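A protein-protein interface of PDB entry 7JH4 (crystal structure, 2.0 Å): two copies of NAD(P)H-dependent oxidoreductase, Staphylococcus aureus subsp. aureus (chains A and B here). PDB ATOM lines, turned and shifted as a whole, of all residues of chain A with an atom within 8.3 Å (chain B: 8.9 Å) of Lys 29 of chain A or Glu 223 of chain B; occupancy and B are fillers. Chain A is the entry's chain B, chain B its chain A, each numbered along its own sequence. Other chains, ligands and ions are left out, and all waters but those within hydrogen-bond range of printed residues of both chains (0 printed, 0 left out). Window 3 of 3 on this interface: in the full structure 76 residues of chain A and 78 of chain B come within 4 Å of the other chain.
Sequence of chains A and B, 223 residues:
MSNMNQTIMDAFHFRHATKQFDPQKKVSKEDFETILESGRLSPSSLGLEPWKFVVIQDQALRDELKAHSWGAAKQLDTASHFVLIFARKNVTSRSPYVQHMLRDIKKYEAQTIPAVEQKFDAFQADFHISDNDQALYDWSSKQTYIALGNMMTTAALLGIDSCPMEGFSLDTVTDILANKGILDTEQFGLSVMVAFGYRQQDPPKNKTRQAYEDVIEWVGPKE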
ATOM      1  N   LYS A  26      -5.092  -1.883  -9.490  1.00  0.00           N
ATOM      2  CA  LYS A  26      -6.272  -2.524  -8.919  1.00  0.00           C
ATOM      3  C   LYS A  26      -6.761  -3.670  -9.797  1.00  0.00           C
ATOM      4  O   LYS A  26      -6.797  -3.554 -11.027  1.00  0.00           O
ATOM      5  CB  LYS A  26      -7.405  -1.513  -8.738  1.00  0.00           C
ATOM      6  CG  LYS A  26      -7.077  -0.396  -7.789  1.00  0.00           C
ATOM      7  CD  LYS A  26      -6.627  -0.910  -6.433  1.00  0.00           C
ATOM      8  CE  LYS A  26      -6.115   0.250  -5.590  1.00  0.00           C
ATOM      9  NZ  LYS A  26      -5.640  -0.191  -4.257  1.00  0.00           N
ATOM     10  N   VAL A  27      -7.138  -4.779  -9.158  1.00  0.00           N
ATOM     11  CA  VAL A  27      -7.793  -5.864  -9.873  1.00  0.00           C
ATOM     12  C   VAL A  27      -9.149  -5.379 -10.372  1.00  0.00           C
ATOM     13  O   VAL A  27      -9.861  -4.657  -9.664  1.00  0.00           O
ATOM     14  CB  VAL A  27      -7.938  -7.096  -8.963  1.00  0.00           C
ATOM     15  CG1 VAL A  27      -8.779  -8.170  -9.634  1.00  0.00           C
ATOM     16  CG2 VAL A  27      -6.565  -7.655  -8.593  1.00  0.00           C
ATOM     17  N   SER A  28      -9.510  -5.753 -11.600  1.00  0.00           N
ATOM     18  CA  SER A  28     -10.808  -5.341 -12.131  1.00  0.00           C
ATOM     19  C   SER A  28     -11.929  -6.078 -11.399  1.00  0.00           C
ATOM     20  O   SER A  28     -11.726  -7.135 -10.796  1.00  0.00           O
ATOM     21  CB  SER A  28     -10.894  -5.616 -13.633  1.00  0.00           C
ATOM     22  OG  SER A  28     -11.131  -6.989 -13.886  1.00  0.00           O
ATOM     23  N   LYS A  29     -13.122  -5.487 -11.435  1.00  0.00           N
ATOM     24  CA  LYS A  29     -14.289  -6.150 -10.862  1.00  0.00           C
ATOM     25  C   LYS A  29     -14.561  -7.474 -11.562  1.00  0.00           C
ATOM     26  O   LYS A  29     -14.811  -8.493 -10.906  1.00  0.00           O
ATOM     27  CB  LYS A  29     -15.505  -5.225 -10.936  1.00  0.00           C
ATOM     28  CG  LYS A  29     -15.369  -3.996 -10.019  1.00  0.00           C
ATOM     29  CD  LYS A  29     -15.917  -2.717 -10.652  1.00  0.00           C
ATOM     30  CE  LYS A  29     -15.099  -1.487 -10.220  1.00  0.00           C
ATOM     31  NZ  LYS A  29     -15.870  -0.199 -10.186  1.00  0.00           N
ATOM     32  N   GLU A  30     -14.495  -7.491 -12.894  1.00  0.00           N
ATOM     33  CA  GLU A  30     -14.669  -8.746 -13.616  1.00  0.00           C
ATOM     34  C   GLU A  30     -13.662  -9.793 -13.144  1.00  0.00           C
ATOM     35  O   GLU A  30     -14.025 -10.944 -12.870  1.00  0.00           O
ATOM     36  CB  GLU A  30     -14.539  -8.508 -15.119  1.00  0.00           C
ATOM     37  N   ASP A  31     -12.385  -9.409 -13.041  1.00  0.00           N
ATOM     38  CA  ASP A  31     -11.366 -10.385 -12.670  1.00  0.00           C
ATOM     39  C   ASP A  31     -11.571 -10.879 -11.244  1.00  0.00           C
ATOM     40  O   ASP A  31     -11.420 -12.077 -10.967  1.00  0.00           O
ATOM     41  CB  ASP A  31      -9.967  -9.792 -12.838  1.00  0.00           C
ATOM     42  CG  ASP A  31      -9.441  -9.921 -14.259  1.00  0.00           C
ATOM     43  OD1 ASP A  31      -9.986 -10.737 -15.040  1.00  0.00           O
ATOM     44  OD2 ASP A  31      -8.466  -9.212 -14.582  1.00  0.00           O
ATOM     45  N   PHE A  32     -11.943  -9.982 -10.329  1.00  0.00           N
ATOM     46  CA  PHE A  32     -12.126 -10.409  -8.949  1.00  0.00           C
ATOM     47  C   PHE A  32     -13.340 -11.315  -8.801  1.00  0.00           C
ATOM     48  O   PHE A  32     -13.326 -12.236  -7.979  1.00  0.00           O
ATOM     49  CB  PHE A  32     -12.252  -9.204  -8.015  1.00  0.00           C
ATOM     50  CG  PHE A  32     -12.107  -9.578  -6.577  1.00  0.00           C
ATOM     51  CD1 PHE A  32     -10.930 -10.157  -6.127  1.00  0.00           C
ATOM     52  CD2 PHE A  32     -13.154  -9.414  -5.686  1.00  0.00           C
ATOM     53  CE1 PHE A  32     -10.784 -10.547  -4.801  1.00  0.00           C
ATOM     54  CE2 PHE A  32     -13.019  -9.799  -4.357  1.00  0.00           C
ATOM     55  CZ  PHE A  32     -11.828 -10.367  -3.917  1.00  0.00           C
ATOM     56  N   GLU A  33     -14.411 -11.067  -9.566  1.00  0.00           N
ATOM     57  CA  GLU A  33     -15.575 -11.939  -9.449  1.00  0.00           C
ATOM     58  C   GLU A  33     -15.222 -13.363  -9.866  1.00  0.00           C
ATOM     59  O   GLU A  33     -15.689 -14.326  -9.246  1.00  0.00           O
ATOM     60  CB  GLU A  33     -16.754 -11.411 -10.259  1.00  0.00           C
ATOM     61  CG  GLU A  33     -17.114  -9.950  -9.965  1.00  0.00           C
ATOM     62  CD  GLU A  33     -17.079  -9.580  -8.473  1.00  0.00           C
ATOM     63  OE1 GLU A  33     -16.391  -8.578  -8.133  1.00  0.00           O
ATOM     64  OE2 GLU A  33     -17.742 -10.268  -7.650  1.00  0.00           O
ATOM     65  N   THR A  34     -14.372 -13.518 -10.895  1.00  0.00           N
ATOM     66  CA  THR A  34     -13.869 -14.847 -11.259  1.00  0.00           C
ATOM     67  C   THR A  34     -13.103 -15.482 -10.104  1.00  0.00           C
ATOM     68  O   THR A  34     -13.285 -16.666  -9.796  1.00  0.00           O
ATOM     69  CB  THR A  34     -12.966 -14.758 -12.497  1.00  0.00           C
ATOM     70  OG1 THR A  34     -13.667 -14.137 -13.571  1.00  0.00           O
ATOM     71  CG2 THR A  34     -12.509 -16.149 -12.937  1.00  0.00           C
ATOM     72  N   ILE A  35     -12.224 -14.708  -9.466  1.00  0.00           N
ATOM     73  CA  ILE A  35     -11.492 -15.204  -8.301  1.00  0.00           C
ATOM     74  C   ILE A  35     -12.462 -15.650  -7.207  1.00  0.00           C
ATOM     75  O   ILE A  35     -12.308 -16.728  -6.617  1.00  0.00           O
ATOM     76  CB  ILE A  35     -10.510 -14.125  -7.799  1.00  0.00           C
ATOM     77  CG1 ILE A  35      -9.435 -13.850  -8.856  1.00  0.00           C
ATOM     78  CG2 ILE A  35      -9.857 -14.548  -6.494  1.00  0.00           C
ATOM     79  CD1 ILE A  35      -8.656 -12.573  -8.598  1.00  0.00           C
ATOM     80  N   LEU A  36     -13.472 -14.823  -6.913  1.00  0.00           N
ATOM     81  CA  LEU A  36     -14.446 -15.179  -5.883  1.00  0.00           C
ATOM     82  C   LEU A  36     -15.235 -16.416  -6.283  1.00  0.00           C
ATOM     83  O   LEU A  36     -15.468 -17.309  -5.460  1.00  0.00           O
ATOM     84  CB  LEU A  36     -15.388 -14.009  -5.633  1.00  0.00           C
ATOM     85  CG  LEU A  36     -14.933 -12.865  -4.725  1.00  0.00           C
ATOM     86  CD1 LEU A  36     -16.030 -11.803  -4.603  1.00  0.00           C
ATOM     87  CD2 LEU A  36     -14.534 -13.375  -3.347  1.00  0.00           C
ATOM     88  N   GLN A  57     -12.100  -4.091   2.111  1.00  0.00           N
ATOM     89  CA  GLN A  57     -11.584  -2.991   1.299  1.00  0.00           C
ATOM     90  C   GLN A  57     -11.432  -1.705   2.101  1.00  0.00           C
ATOM     91  O   GLN A  57     -10.627  -0.842   1.735  1.00  0.00           O
ATOM     92  CB  GLN A  57     -12.482  -2.766   0.081  1.00  0.00           C
ATOM     93  CG  GLN A  57     -12.545  -3.982  -0.859  1.00  0.00           C
ATOM     94  CD  GLN A  57     -11.181  -4.424  -1.349  1.00  0.00           C
ATOM     95  OE1 GLN A  57     -10.456  -5.126  -0.644  1.00  0.00           O
ATOM     96  NE2 GLN A  57     -10.819  -4.013  -2.571  1.00  0.00           N
ATOM     97  N   SER A  80      -4.637  -4.864  -3.658  1.00  0.00           N
ATOM     98  CA  SER A  80      -5.865  -4.370  -4.276  1.00  0.00           C
ATOM     99  C   SER A  80      -7.094  -4.908  -3.546  1.00  0.00           C
ATOM    100  O   SER A  80      -8.006  -4.153  -3.193  1.00  0.00           O
ATOM    101  CB  SER A  80      -5.883  -4.765  -5.758  1.00  0.00           C
ATOM    102  OG  SER A  80      -7.189  -4.731  -6.319  1.00  0.00           O
ATOM    103  N   HIS A  81      -7.125  -6.215  -3.288  1.00  0.00           N
ATOM    104  CA  HIS A  81      -8.238  -6.863  -2.609  1.00  0.00           C
ATOM    105  C   HIS A  81      -7.687  -7.782  -1.529  1.00  0.00           C
ATOM    106  O   HIS A  81      -6.673  -8.464  -1.739  1.00  0.00           O
ATOM    107  CB  HIS A  81      -9.101  -7.683  -3.586  1.00  0.00           C
ATOM    108  CG  HIS A  81      -9.931  -6.850  -4.517  1.00  0.00           C
ATOM    109  ND1 HIS A  81      -9.406  -6.229  -5.632  1.00  0.00           N
ATOM    110  CD2 HIS A  81     -11.253  -6.549  -4.506  1.00  0.00           C
ATOM    111  CE1 HIS A  81     -10.364  -5.571  -6.259  1.00  0.00           C
ATOM    112  NE2 HIS A  81     -11.494  -5.745  -5.594  1.00  0.00           N
ATOM    113  N   ASN B   5     -11.120 -15.882 -18.247  1.00  0.00           N
ATOM    114  CA  ASN B   5     -12.180 -15.963 -17.250  1.00  0.00           C
ATOM    115  C   ASN B   5     -13.155 -17.085 -17.597  1.00  0.00           C
ATOM    116  O   ASN B   5     -13.395 -17.993 -16.790  1.00  0.00           O
ATOM    117  CB  ASN B   5     -12.899 -14.612 -17.144  1.00  0.00           C
ATOM    118  CG  ASN B   5     -11.940 -13.463 -16.833  1.00  0.00           C
ATOM    119  OD1 ASN B   5     -11.172 -13.040 -17.688  1.00  0.00           O
ATOM    120  ND2 ASN B   5     -11.975 -12.969 -15.596  1.00  0.00           N
ATOM    121  N   TYR B 212     -24.337 -16.455  -3.867  1.00  0.00           N
ATOM    122  CA  TYR B 212     -23.226 -15.517  -3.680  1.00  0.00           C
ATOM    123  C   TYR B 212     -23.364 -14.729  -2.383  1.00  0.00           C
ATOM    124  O   TYR B 212     -22.453 -14.704  -1.550  1.00  0.00           O
ATOM    125  CB  TYR B 212     -23.161 -14.569  -4.886  1.00  0.00           C
ATOM    126  CG  TYR B 212     -22.067 -13.502  -4.880  1.00  0.00           C
ATOM    127  CD1 TYR B 212     -22.161 -12.374  -4.061  1.00  0.00           C
ATOM    128  CD2 TYR B 212     -20.964 -13.601  -5.733  1.00  0.00           C
ATOM    129  CE1 TYR B 212     -21.176 -11.387  -4.074  1.00  0.00           C
ATOM    130  CE2 TYR B 212     -19.969 -12.622  -5.754  1.00  0.00           C
ATOM    131  CZ  TYR B 212     -20.080 -11.520  -4.923  1.00  0.00           C
ATOM    132  OH  TYR B 212     -19.109 -10.537  -4.947  1.00  0.00           O
ATOM    133  N   TRP B 218     -18.795  -8.090   1.537  1.00  0.00           N
ATOM    134  CA  TRP B 218     -17.866  -6.983   1.360  1.00  0.00           C
ATOM    135  C   TRP B 218     -17.973  -6.023   2.536  1.00  0.00           C
ATOM    136  O   TRP B 218     -19.074  -5.685   2.983  1.00  0.00           O
ATOM    137  CB  TRP B 218     -18.158  -6.218   0.068  1.00  0.00           C
ATOM    138  CG  TRP B 218     -17.864  -6.980  -1.187  1.00  0.00           C
ATOM    139  CD1 TRP B 218     -18.536  -8.070  -1.672  1.00  0.00           C
ATOM    140  CD2 TRP B 218     -16.828  -6.692  -2.139  1.00  0.00           C
ATOM    141  NE1 TRP B 218     -17.976  -8.482  -2.866  1.00  0.00           N
ATOM    142  CE2 TRP B 218     -16.925  -7.657  -3.172  1.00  0.00           C
ATOM    143  CE3 TRP B 218     -15.827  -5.717  -2.216  1.00  0.00           C
ATOM    144  CZ2 TRP B 218     -16.062  -7.671  -4.268  1.00  0.00           C
ATOM    145  CZ3 TRP B 218     -14.968  -5.730  -3.309  1.00  0.00           C
ATOM    146  CH2 TRP B 218     -15.091  -6.703  -4.320  1.00  0.00           C
ATOM    147  N   GLY B 220     -16.632  -2.314   3.066  1.00  0.00           N
ATOM    148  CA  GLY B 220     -16.013  -1.211   2.370  1.00  0.00           C
ATOM    149  C   GLY B 220     -16.495  -1.129   0.933  1.00  0.00           C
ATOM    150  O   GLY B 220     -17.379  -1.882   0.502  1.00  0.00           O
ATOM    151  N   PRO B 221     -15.917  -0.214   0.156  1.00  0.00           N
ATOM    152  CA  PRO B 221     -16.357  -0.040  -1.237  1.00  0.00           C
ATOM    153  C   PRO B 221     -16.318  -1.354  -2.006  1.00  0.00           C
ATOM    154  O   PRO B 221     -15.340  -2.103  -1.948  1.00  0.00           O
ATOM    155  CB  PRO B 221     -15.358   0.974  -1.799  1.00  0.00           C
ATOM    156  CG  PRO B 221     -14.843   1.715  -0.599  1.00  0.00           C
ATOM    157  CD  PRO B 221     -14.824   0.707   0.517  1.00  0.00           C
ATOM    158  N   LYS B 222     -17.391  -1.634  -2.739  1.00  0.00           N
ATOM    159  CA  LYS B 222     -17.480  -2.860  -3.521  1.00  0.00           C
ATOM    160  C   LYS B 222     -16.919  -2.700  -4.932  1.00  0.00           C
ATOM    161  O   LYS B 222     -16.933  -3.666  -5.704  1.00  0.00           O
ATOM    162  CB  LYS B 222     -18.935  -3.341  -3.579  1.00  0.00           C
ATOM    163  CG  LYS B 222     -19.125  -4.712  -4.213  1.00  0.00           C
ATOM    164  CD  LYS B 222     -20.564  -5.187  -4.069  1.00  0.00           C
ATOM    165  CE  LYS B 222     -20.713  -6.638  -4.487  1.00  0.00           C
ATOM    166  NZ  LYS B 222     -22.122  -7.112  -4.370  1.00  0.00           N
ATOM    167  N   GLU B 223     -16.421  -1.518  -5.282  1.00  0.00           N
ATOM    168  CA  GLU B 223     -15.879  -1.284  -6.616  1.00  0.00           C
ATOM    169  C   GLU B 223     -14.975  -0.051  -6.634  1.00  0.00           C
ATOM    170  O   GLU B 223     -14.736   0.543  -7.685  1.00  0.00           O
ATOM    171  CB  GLU B 223     -17.014  -1.125  -7.631  1.00  0.00           C
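The side-chain amino group of Lys 29 of chain A sits at hydrogen-bond distance from the backbone carbonyl oxygen of Glu 223 of chain B.
The side-chain carboxylate (OD1) of Asp 31 of chain A is in hydrogen-bond range of the side-chain amide nitrogen (ND2) of Asn 5 of chain B (3.0 Å).
The side-chain hydroxyl (OG1) of Thr 34 of chain A lies within hydrogen-bond range of the side-chain amide nitrogen (ND2) of Asn 5 of chain B.
The side-chain carboxylate of Glu 33 of chain A is in hydrogen-bond range of the side-chain hydroxyl of Tyr 212 of chain B (3.0 Å).
OH of Tyr 212 of chain B sits at hydrogen-bond distance from NE1 of Trp 218 of chain B.
The side-chain hydroxyl of Ser 28 of chain A lies within hydrogen-bond range of the backbone NH of Asp 31 of chain A, 2.9 Å away.
NE2 of Gln 57 of chain A sits at hydrogen-bond distance from O of Ser 80 of chain A (2.9 Å).
O of Glu 30 of chain A is in hydrogen-bond range of OG1 of Thr 34 of chain A (3.3 Å).
The side-chain hydroxyl (OG) of Ser 80 of chain A is in hydrogen-bond range of a ring nitrogen (ND1) of His 81 of chain A (2.8 Å).
Among the printed residues, pairs that only touch across the chains: Leu 36 of chain A with Tyr 212 of chain B (3.3 Å), Gln 57 of chain A with Pro 221 of chain B (3.5 Å), Phe 32 of chain A with Trp 218 of chain B (3.6 Å), His 81 of chain A with Trp 218 of chain B (3.8 Å), Gln 57 of chain A with Trp 218 of chain B (3.9 Å), Glu 30 of chain A with Asn 5 of chain B (3.97 Å) and Glu 33 of chain A with Trp 218 of chain B (3.98 Å).
Ser 28 of chain A touches none of the printed residues of chain B.
Lys 29 of chain A touches just one residue of chain B: Glu 223 (2.8 Å).
Of chain B, only Asn 5 comes within 4 Å of Glu 30 of chain A.
Printed residues of chain B within 4 Å of His 81 of chain A: Trp 218.
Printed residues of chain A within 4 Å of Asn 5 of chain B: Glu 30 (3.97 Å), Asp 31 (3.0 Å) and Thr 34 (2.9 Å).
Printed residues of chain A within 4 Å of Tyr 212 of chain B: Glu 33 and Leu 36.
Printed residues of chain A within 4 Å of Trp 218 of chain B: Phe 32, Glu 33, Gln 57 and His 81.
Glu 223 of chain B touches one residue of chain A.
The nearest residue of chain B that does not touch Lys 29 of chain A is Lys 222 of chain B (4.6 Å).
The nearest residue of chain A that does not touch Glu 223 of chain B is His 81 of chain A (6.3 Å).
Of the 7 printed residues of chain B, 5 touch a printed residue of chain A.
Hydrophobic or aromatic side chains of chain B within 4 Å of the printed part of chain A: Tyr 212 and Trp 218.
Of the 14 printed residues of chain A, 9 touch a printed residue of chain B.
Hydrophobic or aromatic side chains of chain A within 4 Å of the printed part of chain B: Phe 32, Leu 36 and His 81.
Among the printed residues, 11 pairs touch across the chains.
Among the printed residues, no Asp or Glu carboxylate lies within 4 Å of a Lys or Arg side-chain nitrogen of the other chain.
No position is printed for both chains.
Of the 11 pairs that touch across the chains among the printed residues, none has its exchanged pair printed and touching as well.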
